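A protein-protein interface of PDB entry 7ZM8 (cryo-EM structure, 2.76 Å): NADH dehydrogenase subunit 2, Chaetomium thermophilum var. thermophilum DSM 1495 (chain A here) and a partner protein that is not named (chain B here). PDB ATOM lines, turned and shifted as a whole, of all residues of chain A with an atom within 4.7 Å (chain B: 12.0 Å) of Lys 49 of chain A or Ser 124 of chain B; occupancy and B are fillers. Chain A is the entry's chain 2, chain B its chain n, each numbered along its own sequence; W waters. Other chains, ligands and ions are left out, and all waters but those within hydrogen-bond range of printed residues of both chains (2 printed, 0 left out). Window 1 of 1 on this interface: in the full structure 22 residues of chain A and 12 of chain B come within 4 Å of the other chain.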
ATOM      1  N   ILE A  47     -27.945 -36.399  14.853  1.00  0.00           N
ATOM      2  CA  ILE A  47     -27.898 -36.197  13.382  1.00  0.00           C
ATOM      3  C   ILE A  47     -28.276 -34.737  13.170  1.00  0.00           C
ATOM      4  O   ILE A  47     -29.418 -34.376  13.437  1.00  0.00           O
ATOM      5  CB  ILE A  47     -28.865 -37.144  12.662  1.00  0.00           C
ATOM      6  CG1 ILE A  47     -28.376 -38.587  12.734  1.00  0.00           C
ATOM      7  CG2 ILE A  47     -29.069 -36.706  11.222  1.00  0.00           C
ATOM      8  CD1 ILE A  47     -26.940 -38.738  12.319  1.00  0.00           C
ATOM      9  N   SER A  48     -27.314 -33.917  12.752  1.00  0.00           N
ATOM     10  CA  SER A  48     -27.586 -32.466  12.642  1.00  0.00           C
ATOM     11  C   SER A  48     -26.677 -31.867  11.585  1.00  0.00           C
ATOM     12  O   SER A  48     -25.487 -32.221  11.565  1.00  0.00           O
ATOM     13  CB  SER A  48     -27.342 -31.791  13.966  1.00  0.00           C
ATOM     14  OG  SER A  48     -27.582 -30.395  13.875  1.00  0.00           O
ATOM     15  N   LYS A  49     -27.221 -30.992  10.746  1.00  0.00           N
ATOM     16  CA  LYS A  49     -26.351 -30.275   9.787  1.00  0.00           C
ATOM     17  C   LYS A  49     -25.406 -29.403  10.620  1.00  0.00           C
ATOM     18  O   LYS A  49     -24.282 -29.172  10.180  1.00  0.00           O
ATOM     19  CB  LYS A  49     -27.186 -29.578   8.715  1.00  0.00           C
ATOM     20  CG  LYS A  49     -28.191 -30.490   8.028  1.00  0.00           C
ATOM     21  CD  LYS A  49     -28.845 -29.881   6.816  1.00  0.00           C
ATOM     22  CE  LYS A  49     -27.840 -29.453   5.773  1.00  0.00           C
ATOM     23  NZ  LYS A  49     -28.437 -29.449   4.418  1.00  0.00           N
ATOM     24  N   GLY A  50     -25.860 -28.922  11.778  1.00  0.00           N
ATOM     25  CA  GLY A  50     -24.972 -28.154  12.663  1.00  0.00           C
ATOM     26  C   GLY A  50     -25.692 -27.562  13.856  1.00  0.00           C
ATOM     27  O   GLY A  50     -26.893 -27.288  13.737  1.00  0.00           O
ATOM     28  N   THR A  61     -20.761 -30.298  14.132  1.00  0.00           N
ATOM     29  CA  THR A  61     -21.418 -31.072  13.054  1.00  0.00           C
ATOM     30  C   THR A  61     -20.857 -32.469  13.233  1.00  0.00           C
ATOM     31  O   THR A  61     -19.853 -32.584  13.931  1.00  0.00           O
ATOM     32  CB  THR A  61     -21.107 -30.451  11.681  1.00  0.00           C
ATOM     33  OG1 THR A  61     -21.585 -29.107  11.622  1.00  0.00           O
ATOM     34  CG2 THR A  61     -21.670 -31.225  10.513  1.00  0.00           C
ATOM     35  N   TYR A 296     -20.471 -25.640  -0.128  1.00  0.00           N
ATOM     36  CA  TYR A 296     -21.850 -26.171  -0.176  1.00  0.00           C
ATOM     37  C   TYR A 296     -22.918 -25.093  -0.058  1.00  0.00           C
ATOM     38  O   TYR A 296     -23.882 -25.142  -0.821  1.00  0.00           O
ATOM     39  CB  TYR A 296     -22.076 -27.159   0.973  1.00  0.00           C
ATOM     40  CG  TYR A 296     -23.441 -27.789   0.972  1.00  0.00           C
ATOM     41  CD1 TYR A 296     -23.714 -28.873   0.159  1.00  0.00           C
ATOM     42  CD2 TYR A 296     -24.468 -27.286   1.750  1.00  0.00           C
ATOM     43  CE1 TYR A 296     -24.970 -29.447   0.122  1.00  0.00           C
ATOM     44  CE2 TYR A 296     -25.732 -27.845   1.721  1.00  0.00           C
ATOM     45  CZ  TYR A 296     -25.983 -28.928   0.900  1.00  0.00           C
ATOM     46  OH  TYR A 296     -27.217 -29.499   0.863  1.00  0.00           O
ATOM     47  N   TYR A 297     -22.781 -24.174   0.889  1.00  0.00           N
ATOM     48  CA  TYR A 297     -23.859 -23.186   1.142  1.00  0.00           C
ATOM     49  C   TYR A 297     -23.641 -21.934   0.310  1.00  0.00           C
ATOM     50  O   TYR A 297     -24.410 -20.991   0.500  1.00  0.00           O
ATOM     51  CB  TYR A 297     -23.915 -22.793   2.615  1.00  0.00           C
ATOM     52  CG  TYR A 297     -24.295 -23.874   3.591  1.00  0.00           C
ATOM     53  CD1 TYR A 297     -25.613 -24.258   3.753  1.00  0.00           C
ATOM     54  CD2 TYR A 297     -23.341 -24.479   4.388  1.00  0.00           C
ATOM     55  CE1 TYR A 297     -25.969 -25.240   4.663  1.00  0.00           C
ATOM     56  CE2 TYR A 297     -23.676 -25.462   5.299  1.00  0.00           C
ATOM     57  CZ  TYR A 297     -24.997 -25.844   5.438  1.00  0.00           C
ATOM     58  OH  TYR A 297     -25.340 -26.812   6.335  1.00  0.00           O
ATOM     59  N   ASN A 301     -28.207 -22.849  -7.129  1.00  0.00           N
ATOM     60  CA  ASN A 301     -29.186 -23.909  -7.483  1.00  0.00           C
ATOM     61  C   ASN A 301     -29.926 -23.420  -8.727  1.00  0.00           C
ATOM     62  O   ASN A 301     -30.629 -24.231  -9.358  1.00  0.00           O
ATOM     63  CB  ASN A 301     -30.109 -24.238  -6.309  1.00  0.00           C
ATOM     64  CG  ASN A 301     -29.347 -24.641  -5.062  1.00  0.00           C
ATOM     65  OD1 ASN A 301     -28.321 -25.313  -5.144  1.00  0.00           O
ATOM     66  ND2 ASN A 301     -29.844 -24.238  -3.904  1.00  0.00           N
ATOM     67  N   ILE A 567     -26.029 -36.362   5.416  1.00  0.00           N
ATOM     68  CA  ILE A 567     -26.501 -35.320   6.374  1.00  0.00           C
ATOM     69  C   ILE A 567     -26.275 -33.917   5.807  1.00  0.00           C
ATOM     70  O   ILE A 567     -27.178 -33.097   5.899  1.00  0.00           O
ATOM     71  CB  ILE A 567     -25.865 -35.511   7.766  1.00  0.00           C
ATOM     72  CG1 ILE A 567     -26.057 -36.934   8.296  1.00  0.00           C
ATOM     73  CG2 ILE A 567     -26.363 -34.474   8.754  1.00  0.00           C
ATOM     74  CD1 ILE A 567     -25.128 -37.291   9.431  1.00  0.00           C
ATOM     75  N   LEU A 568     -25.120 -33.664   5.210  1.00  0.00           N
ATOM     76  CA  LEU A 568     -24.785 -32.326   4.663  1.00  0.00           C
ATOM     77  C   LEU A 568     -25.731 -31.952   3.526  1.00  0.00           C
ATOM     78  O   LEU A 568     -26.137 -30.803   3.486  1.00  0.00           O
ATOM     79  CB  LEU A 568     -23.338 -32.378   4.165  1.00  0.00           C
ATOM     80  CG  LEU A 568     -22.887 -31.199   3.305  1.00  0.00           C
ATOM     81  CD1 LEU A 568     -22.887 -29.906   4.100  1.00  0.00           C
ATOM     82  CD2 LEU A 568     -21.514 -31.461   2.712  1.00  0.00           C
ATOM     83  N   PHE A 569     -26.042 -32.888   2.638  1.00  0.00           N
ATOM     84  CA  PHE A 569     -26.906 -32.619   1.462  1.00  0.00           C
ATOM     85  C   PHE A 569     -28.365 -32.836   1.843  1.00  0.00           C
ATOM     86  O   PHE A 569     -29.217 -32.282   1.147  1.00  0.00           O
ATOM     87  CB  PHE A 569     -26.478 -33.531   0.313  1.00  0.00           C
ATOM     88  CG  PHE A 569     -25.370 -32.994  -0.557  1.00  0.00           C
ATOM     89  CD1 PHE A 569     -24.062 -32.964  -0.108  1.00  0.00           C
ATOM     90  CD2 PHE A 569     -25.633 -32.534  -1.836  1.00  0.00           C
ATOM     91  CE1 PHE A 569     -23.045 -32.473  -0.907  1.00  0.00           C
ATOM     92  CE2 PHE A 569     -24.615 -32.046  -2.638  1.00  0.00           C
ATOM     93  CZ  PHE A 569     -23.325 -32.012  -2.171  1.00  0.00           C
ATOM     94  N   SER A 570     -28.622 -33.521   2.958  1.00  0.00           N
ATOM     95  CA  SER A 570     -29.995 -33.920   3.361  1.00  0.00           C
ATOM     96  C   SER A 570     -30.950 -32.741   3.415  1.00  0.00           C
ATOM     97  O   SER A 570     -30.495 -31.639   3.770  1.00  0.00           O
ATOM     98  CB  SER A 570     -30.006 -34.584   4.677  1.00  0.00           C
ATOM     99  OG  SER A 570     -29.740 -33.646   5.707  1.00  0.00           O
ATOM    100  N   ALA A 571     -32.227 -33.007   3.129  1.00  0.00           N
ATOM    101  CA  ALA A 571     -33.235 -31.934   3.027  1.00  0.00           C
ATOM    102  C   ALA A 571     -32.796 -31.061   1.857  1.00  0.00           C
ATOM    103  O   ALA A 571     -32.515 -31.658   0.807  1.00  0.00           O
ATOM    104  CB  ALA A 571     -33.379 -31.170   4.322  1.00  0.00           C
ATOM    105  N   LEU B 117     -30.017 -43.920  -5.944  1.00  0.00           N
ATOM    106  CA  LEU B 117     -30.923 -43.133  -5.063  1.00  0.00           C
ATOM    107  C   LEU B 117     -30.121 -42.213  -4.142  1.00  0.00           C
ATOM    108  O   LEU B 117     -30.468 -41.040  -4.039  1.00  0.00           O
ATOM    109  CB  LEU B 117     -31.774 -44.118  -4.258  1.00  0.00           C
ATOM    110  CG  LEU B 117     -32.819 -43.508  -3.330  1.00  0.00           C
ATOM    111  CD1 LEU B 117     -33.998 -42.974  -4.127  1.00  0.00           C
ATOM    112  CD2 LEU B 117     -33.283 -44.533  -2.313  1.00  0.00           C
ATOM    113  N   LEU B 118     -29.058 -42.729  -3.530  1.00  0.00           N
ATOM    114  CA  LEU B 118     -28.256 -41.933  -2.571  1.00  0.00           C
ATOM    115  C   LEU B 118     -27.414 -40.885  -3.304  1.00  0.00           C
ATOM    116  O   LEU B 118     -27.243 -39.796  -2.746  1.00  0.00           O
ATOM    117  CB  LEU B 118     -27.371 -42.888  -1.770  1.00  0.00           C
ATOM    118  CG  LEU B 118     -28.076 -43.766  -0.741  1.00  0.00           C
ATOM    119  CD1 LEU B 118     -27.220 -44.975  -0.399  1.00  0.00           C
ATOM    120  CD2 LEU B 118     -28.399 -42.976   0.515  1.00  0.00           C
ATOM    121  N   LEU B 119     -26.926 -41.191  -4.505  1.00  0.00           N
ATOM    122  CA  LEU B 119     -25.997 -40.269  -5.215  1.00  0.00           C
ATOM    123  C   LEU B 119     -26.744 -39.216  -6.038  1.00  0.00           C
ATOM    124  O   LEU B 119     -26.074 -38.294  -6.527  1.00  0.00           O
ATOM    125  CB  LEU B 119     -25.074 -41.107  -6.104  1.00  0.00           C
ATOM    126  CG  LEU B 119     -23.573 -40.925  -5.898  1.00  0.00           C
ATOM    127  CD1 LEU B 119     -23.215 -40.995  -4.426  1.00  0.00           C
ATOM    128  CD2 LEU B 119     -22.806 -41.976  -6.680  1.00  0.00           C
ATOM    129  N   THR B 120     -28.056 -39.357  -6.221  1.00  0.00           N
ATOM    130  CA  THR B 120     -28.799 -38.409  -7.093  1.00  0.00           C
ATOM    131  C   THR B 120     -29.899 -37.764  -6.264  1.00  0.00           C
ATOM    132  O   THR B 120     -30.997 -37.566  -6.808  1.00  0.00           O
ATOM    133  CB  THR B 120     -29.410 -39.078  -8.333  1.00  0.00           C
ATOM    134  OG1 THR B 120     -30.412 -40.009  -7.925  1.00  0.00           O
ATOM    135  CG2 THR B 120     -28.394 -39.754  -9.225  1.00  0.00           C
ATOM    136  N   ALA B 121     -29.592 -37.401  -5.021  1.00  0.00           N
ATOM    137  CA  ALA B 121     -30.644 -36.898  -4.132  1.00  0.00           C
ATOM    138  C   ALA B 121     -30.716 -35.377  -4.172  1.00  0.00           C
ATOM    139  O   ALA B 121     -29.720 -34.752  -4.522  1.00  0.00           O
ATOM    140  CB  ALA B 121     -30.440 -37.470  -2.753  1.00  0.00           C
ATOM    141  N   GLU B 122     -31.888 -34.825  -3.868  1.00  0.00           N
ATOM    142  CA  GLU B 122     -32.075 -33.361  -3.941  1.00  0.00           C
ATOM    143  C   GLU B 122     -31.162 -32.677  -2.920  1.00  0.00           C
ATOM    144  O   GLU B 122     -31.148 -33.095  -1.770  1.00  0.00           O
ATOM    145  CB  GLU B 122     -33.548 -33.029  -3.715  1.00  0.00           C
ATOM    146  CG  GLU B 122     -33.879 -31.556  -3.860  1.00  0.00           C
ATOM    147  CD  GLU B 122     -33.843 -31.019  -5.281  1.00  0.00           C
ATOM    148  OE1 GLU B 122     -33.894 -31.834  -6.224  1.00  0.00           O
ATOM    149  OE2 GLU B 122     -33.766 -29.785  -5.442  1.00  0.00           O
ATOM    150  N   ARG B 123     -30.436 -31.656  -3.350  1.00  0.00           N
ATOM    151  CA  ARG B 123     -29.578 -30.879  -2.433  1.00  0.00           C
ATOM    152  C   ARG B 123     -30.511 -29.909  -1.729  1.00  0.00           C
ATOM    153  O   ARG B 123     -31.457 -29.441  -2.373  1.00  0.00           O
ATOM    154  CB  ARG B 123     -28.558 -30.089  -3.262  1.00  0.00           C
ATOM    155  CG  ARG B 123     -27.496 -29.340  -2.480  1.00  0.00           C
ATOM    156  CD  ARG B 123     -26.810 -28.380  -3.429  1.00  0.00           C
ATOM    157  NE  ARG B 123     -25.541 -27.893  -2.916  1.00  0.00           N
ATOM    158  CZ  ARG B 123     -24.358 -28.287  -3.361  1.00  0.00           C
ATOM    159  NH1 ARG B 123     -24.280 -29.158  -4.351  1.00  0.00           N
ATOM    160  NH2 ARG B 123     -23.258 -27.795  -2.828  1.00  0.00           N
ATOM    161  N   SER B 124     -30.245 -29.629  -0.460  1.00  0.00           N
ATOM    162  CA  SER B 124     -31.065 -28.662   0.294  1.00  0.00           C
ATOM    163  C   SER B 124     -30.961 -27.294  -0.355  1.00  0.00           C
ATOM    164  O   SER B 124     -29.847 -26.884  -0.705  1.00  0.00           O
ATOM    165  CB  SER B 124     -30.631 -28.606   1.707  1.00  0.00           C
ATOM    166  OG  SER B 124     -29.292 -28.158   1.798  1.00  0.00           O
ATOM    167  N   ARG B 125     -32.099 -26.647  -0.542  1.00  0.00           N
ATOM    168  CA  ARG B 125     -32.091 -25.268  -1.053  1.00  0.00           C
ATOM    169  C   ARG B 125     -32.563 -24.417   0.120  1.00  0.00           C
ATOM    170  O   ARG B 125     -32.636 -23.188  -0.026  1.00  0.00           O
ATOM    171  CB  ARG B 125     -33.019 -25.156  -2.262  1.00  0.00           C
ATOM    172  CG  ARG B 125     -32.781 -26.210  -3.334  1.00  0.00           C
ATOM    173  CD  ARG B 125     -33.652 -25.941  -4.543  1.00  0.00           C
ATOM    174  NE  ARG B 125     -33.347 -24.644  -5.129  1.00  0.00           N
ATOM    175  CZ  ARG B 125     -34.009 -24.104  -6.143  1.00  0.00           C
ATOM    176  NH1 ARG B 125     -35.026 -24.750  -6.687  1.00  0.00           N
ATOM    177  NH2 ARG B 125     -33.655 -22.921  -6.610  1.00  0.00           N
ATOM    178  N   HIS B 126     -32.838 -25.070   1.245  1.00  0.00           N
ATOM    179  CA  HIS B 126     -33.286 -24.357   2.459  1.00  0.00           C
ATOM    180  C   HIS B 126     -32.174 -24.401   3.497  1.00  0.00           C
ATOM    181  O   HIS B 126     -31.565 -25.456   3.657  1.00  0.00           O
ATOM    182  CB  HIS B 126     -34.570 -25.001   2.976  1.00  0.00           C
ATOM    183  CG  HIS B 126     -35.024 -24.511   4.306  1.00  0.00           C
ATOM    184  ND1 HIS B 126     -35.256 -23.181   4.557  1.00  0.00           N
ATOM    185  CD2 HIS B 126     -35.318 -25.171   5.443  1.00  0.00           C
ATOM    186  CE1 HIS B 126     -35.657 -23.039   5.799  1.00  0.00           C
ATOM    187  NE2 HIS B 126     -35.711 -24.243   6.362  1.00  0.00           N
ATOM    188  N   ILE B 127     -31.945 -23.293   4.189  1.00  0.00           N
ATOM    189  CA  ILE B 127     -30.940 -23.276   5.282  1.00  0.00           C
ATOM    190  C   ILE B 127     -31.702 -23.281   6.602  1.00  0.00           C
ATOM    191  O   ILE B 127     -32.661 -22.525   6.712  1.00  0.00           O
ATOM    192  CB  ILE B 127     -30.042 -22.032   5.134  1.00  0.00           C
ATOM    193  CG1 ILE B 127     -29.107 -22.169   3.934  1.00  0.00           C
ATOM    194  CG2 ILE B 127     -29.271 -21.748   6.414  1.00  0.00           C
ATOM    195  CD1 ILE B 127     -28.821 -20.871   3.242  1.00  0.00           C
ATOM    196  N   GLU B 128     -31.310 -24.132   7.539  1.00  0.00           N
ATOM    197  CA  GLU B 128     -31.914 -24.133   8.889  1.00  0.00           C
ATOM    198  C   GLU B 128     -30.862 -23.502   9.795  1.00  0.00           C
ATOM    199  O   GLU B 128     -29.691 -23.880   9.687  1.00  0.00           O
ATOM    200  CB  GLU B 128     -32.331 -25.538   9.323  1.00  0.00           C
ATOM    201  CG  GLU B 128     -31.199 -26.544   9.378  1.00  0.00           C
ATOM    202  CD  GLU B 128     -31.642 -27.988   9.526  1.00  0.00           C
ATOM    203  OE1 GLU B 128     -30.769 -28.857   9.724  1.00  0.00           O
ATOM    204  OE2 GLU B 128     -32.858 -28.243   9.438  1.00  0.00           O
ATOM    205  N   LEU B 129     -31.255 -22.522  10.597  1.00  0.00           N
ATOM    206  CA  LEU B 129     -30.263 -21.804  11.416  1.00  0.00           C
ATOM    207  C   LEU B 129     -29.664 -22.772  12.428  1.00  0.00           C
ATOM    208  O   LEU B 129     -30.437 -23.439  13.121  1.00  0.00           O
ATOM    209  CB  LEU B 129     -30.967 -20.618  12.077  1.00  0.00           C
ATOM    210  CG  LEU B 129     -31.385 -19.500  11.130  1.00  0.00           C
ATOM    211  CD1 LEU B 129     -32.312 -18.527  11.834  1.00  0.00           C
ATOM    212  CD2 LEU B 129     -30.160 -18.779  10.596  1.00  0.00           C
ATOM    213  N   LYS B 130     -28.334 -22.824  12.512  1.00  0.00           N
ATOM    214  CA  LYS B 130     -27.634 -23.694  13.487  1.00  0.00           C
ATOM    215  C   LYS B 130     -27.855 -23.049  14.847  1.00  0.00           C
ATOM    216  O   LYS B 130     -27.917 -23.776  15.840  1.00  0.00           O
ATOM    217  CB  LYS B 130     -26.146 -23.735  13.128  1.00  0.00           C
ATOM    218  CG  LYS B 130     -25.774 -24.495  11.865  1.00  0.00           C
ATOM    219  CD  LYS B 130     -24.290 -24.455  11.587  1.00  0.00           C
ATOM    220  CE  LYS B 130     -23.860 -25.396  10.483  1.00  0.00           C
ATOM    221  NZ  LYS B 130     -24.670 -25.220   9.256  1.00  0.00           N
ATOM    222  N   TYR B 131     -28.082 -21.732  14.843  1.00  0.00           N
ATOM    223  CA  TYR B 131     -28.254 -20.928  16.078  1.00  0.00           C
ATOM    224  C   TYR B 131     -29.546 -20.103  15.995  1.00  0.00           C
ATOM    225  O   TYR B 131     -29.468 -18.885  15.779  1.00  0.00           O
ATOM    226  CB  TYR B 131     -26.984 -20.106  16.305  1.00  0.00           C
ATOM    227  CG  TYR B 131     -26.917 -19.284  17.564  1.00  0.00           C
ATOM    228  CD1 TYR B 131     -26.863 -19.880  18.812  1.00  0.00           C
ATOM    229  CD2 TYR B 131     -26.855 -17.903  17.500  1.00  0.00           C
ATOM    230  CE1 TYR B 131     -26.781 -19.122  19.967  1.00  0.00           C
ATOM    231  CE2 TYR B 131     -26.776 -17.130  18.643  1.00  0.00           C
ATOM    232  CZ  TYR B 131     -26.740 -17.743  19.880  1.00  0.00           C
ATOM    233  OH  TYR B 131     -26.650 -16.980  21.006  1.00  0.00           O
ATOM    234  N   PRO B 132     -30.746 -20.712  16.128  1.00  0.00           N
ATOM    235  CA  PRO B 132     -32.026 -19.978  16.129  1.00  0.00           C
ATOM    236  C   PRO B 132     -32.128 -18.980  17.291  1.00  0.00           C
ATOM    237  O   PRO B 132     -33.007 -18.163  17.256  1.00  0.00           O
ATOM    238  CB  PRO B 132     -33.073 -21.072  16.382  1.00  0.00           C
ATOM    239  CG  PRO B 132     -32.299 -22.213  16.969  1.00  0.00           C
ATOM    240  CD  PRO B 132     -30.958 -22.149  16.278  1.00  0.00           C
ATOM    241  N   GLN B 161     -41.817 -27.149  15.903  1.00  0.00           N
ATOM    242  CA  GLN B 161     -40.698 -28.060  15.566  1.00  0.00           C
ATOM    243  C   GLN B 161     -40.281 -28.891  16.773  1.00  0.00           C
ATOM    244  O   GLN B 161     -40.062 -30.098  16.600  1.00  0.00           O
ATOM    245  CB  GLN B 161     -39.567 -27.224  14.976  1.00  0.00           C
ATOM    246  CG  GLN B 161     -38.297 -27.994  14.670  1.00  0.00           C
ATOM    247  CD  GLN B 161     -37.237 -27.063  14.145  1.00  0.00           C
ATOM    248  OE1 GLN B 161     -37.498 -25.893  13.891  1.00  0.00           O
ATOM    249  NE2 GLN B 161     -36.033 -27.579  13.971  1.00  0.00           N
ATOM    250  N   GLU B 165     -40.720 -33.171  17.002  1.00  0.00           N
ATOM    251  CA  GLU B 165     -39.630 -34.124  17.315  1.00  0.00           C
ATOM    252  C   GLU B 165     -39.919 -34.891  18.608  1.00  0.00           C
ATOM    253  O   GLU B 165     -39.626 -36.083  18.652  1.00  0.00           O
ATOM    254  CB  GLU B 165     -38.264 -33.439  17.252  1.00  0.00           C
ATOM    255  CG  GLU B 165     -37.114 -34.270  17.780  1.00  0.00           C
ATOM    256  CD  GLU B 165     -36.247 -34.910  16.712  1.00  0.00           C
ATOM    257  OE1 GLU B 165     -36.482 -34.642  15.520  1.00  0.00           O
ATOM    258  OE2 GLU B 165     -35.337 -35.677  17.079  1.00  0.00           O
HETATM  259  O   HOH W   1     -31.507 -34.770   0.065  1.00  0.00           O
HETATM  260  O   HOH W   2     -26.323 -26.033  -0.993  1.00  0.00           O
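The backbone carbonyl oxygen (O) of Ala 571 of chain A lies close to the backbone carbonyl oxygen (O) of Glu 122 of chain B, 3.3 Å away. The side-chain hydroxyl (OH) of Tyr 297 of chain A is in hydrogen-bond range of the side-chain amino group (NZ) of Lys 130 of chain B (3.4 Å). The side-chain hydroxyl (OH) of Tyr 296 of chain A lies within hydrogen-bond range of the side-chain hydroxyl (OG) of Ser 124 of chain B (2.6 Å). The backbone carbonyl oxygen of Phe 569 of chain A lies within hydrogen-bond range of the backbone NH of Ser 124 of chain B, at 3.3 Å. The backbone carbonyl oxygen of Ala 571 of chain A lies within hydrogen-bond range of the backbone NH of Ser 124 of chain B (3.3 Å). NH2 of Arg 123 of chain B lies close to O of Tyr 296 of chain A (3.4 Å). NZ of Lys 49 of chain A lies within hydrogen-bond range of OG of Ser 124 of chain B, at 3.0 Å.
Water W1 lies within hydrogen-bond range of the backbone carbonyl oxygen of Glu 122 of chain B (2.5 Å) and the backbone carbonyl oxygen of Ala 571 of chain A (3.4 Å). Water W2 lies within hydrogen-bond range of the backbone carbonyl oxygen (O) of Tyr 296 of chain A and the guanidinium group (NE) of Arg 123 of chain B.
OE1 of Glu 128 of chain B touches CG of Lys 49 of chain A, 3.5 Å away. O of Lys 49 of chain A touches CE of Lys 130 of chain B, at 3.8 Å. Lys 130 of chain B touches Gly 50 of chain A (CG to O, 3.5 Å). Asn 301 of chain A touches Arg 123 of chain B (OD1 to CD, 3.8 Å). Arg 125 of chain B touches Asn 301 of chain A. O of Glu 122 of chain B touches O of Phe 569 of chain A, at 3.6 Å. Phe 569 of chain A touches Arg 123 of chain B (CE2 to NH1, 3.4 Å). CB of Ser 124 of chain B touches O of Ser 570 of chain A (3.7 Å). Arg 123 of chain B touches Ala 571 of chain A.
Along chain B the printed residues that touch a printed residue of chain A span positions 122 to 130. Hydrophobic or aromatic side chains of chain A that line the printed part of chain B: Tyr 296, Tyr 297 and Phe 569. Among the printed residues, no Asp or Glu carboxylate lies within 4 Å of a Lys or Arg side-chain nitrogen of the other chain.
Lys 49 of chain A touches just these residues of chain B: Ser 124, Glu 128 and Lys 130. Of chain A, only Lys 49 (3.0 Å), Tyr 296 (2.6 Å), Phe 569 (3.3 Å), Ser 570 (3.7 Å) and Ala 571 (3.3 Å) come within 4 Å of Ser 124 of chain B. Ser 48 of chain A touches none of the printed residues of chain B. No residue of chain B comes within 4 Å of Ile 567 of chain A. Ser 570 of chain A touches just one residue of chain B: Ser 124 (3.7 Å). Of chain B, only Glu 122, Arg 123 and Ser 124 come within 4 Å of Ala 571 of chain A. Of the printed residues of chain A, Arg 125 of chain B touches Asn 301. Printed residues of chain A within 4 Å of Glu 128 of chain B: Lys 49 (3.5 Å). Of the printed residues of chain B, Tyr 297 of chain A touches Lys 130 (3.4 Å). Printed residues of chain A within 4 Å of Arg 123 of chain B: Tyr 296 (3.2 Å), Asn 301 (3.8 Å), Phe 569 (3.4 Å) and Ala 571 (3.7 Å). Ala 121 of chain B touches none of the printed residues of chain A. The nearest residue of chain B that does not touch Lys 49 of chain A is His 126 of chain B (5.1 Å).
O of Ile 567 of chain A lies within hydrogen-bond range of OG of Ser 570 of chain A, at 2.6 Å. NZ of Lys 49 of chain A is in hydrogen-bond range of O of Ser 570 of chain A. OH of Tyr 296 of chain A sits close to O of Phe 569 of chain A (3.4 Å). The side-chain amino group (NZ) of Lys 49 of chain A sits at hydrogen-bond distance from the backbone carbonyl oxygen (O) of Leu 568 of chain A (2.8 Å). The backbone carbonyl oxygen of Lys 49 of chain A is in hydrogen-bond range of the side-chain hydroxyl of Thr 61 of chain A, at 3.1 Å. OG of Ser 48 of chain A sits close to N of Gly 50 of chain A, at 3.1 Å.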
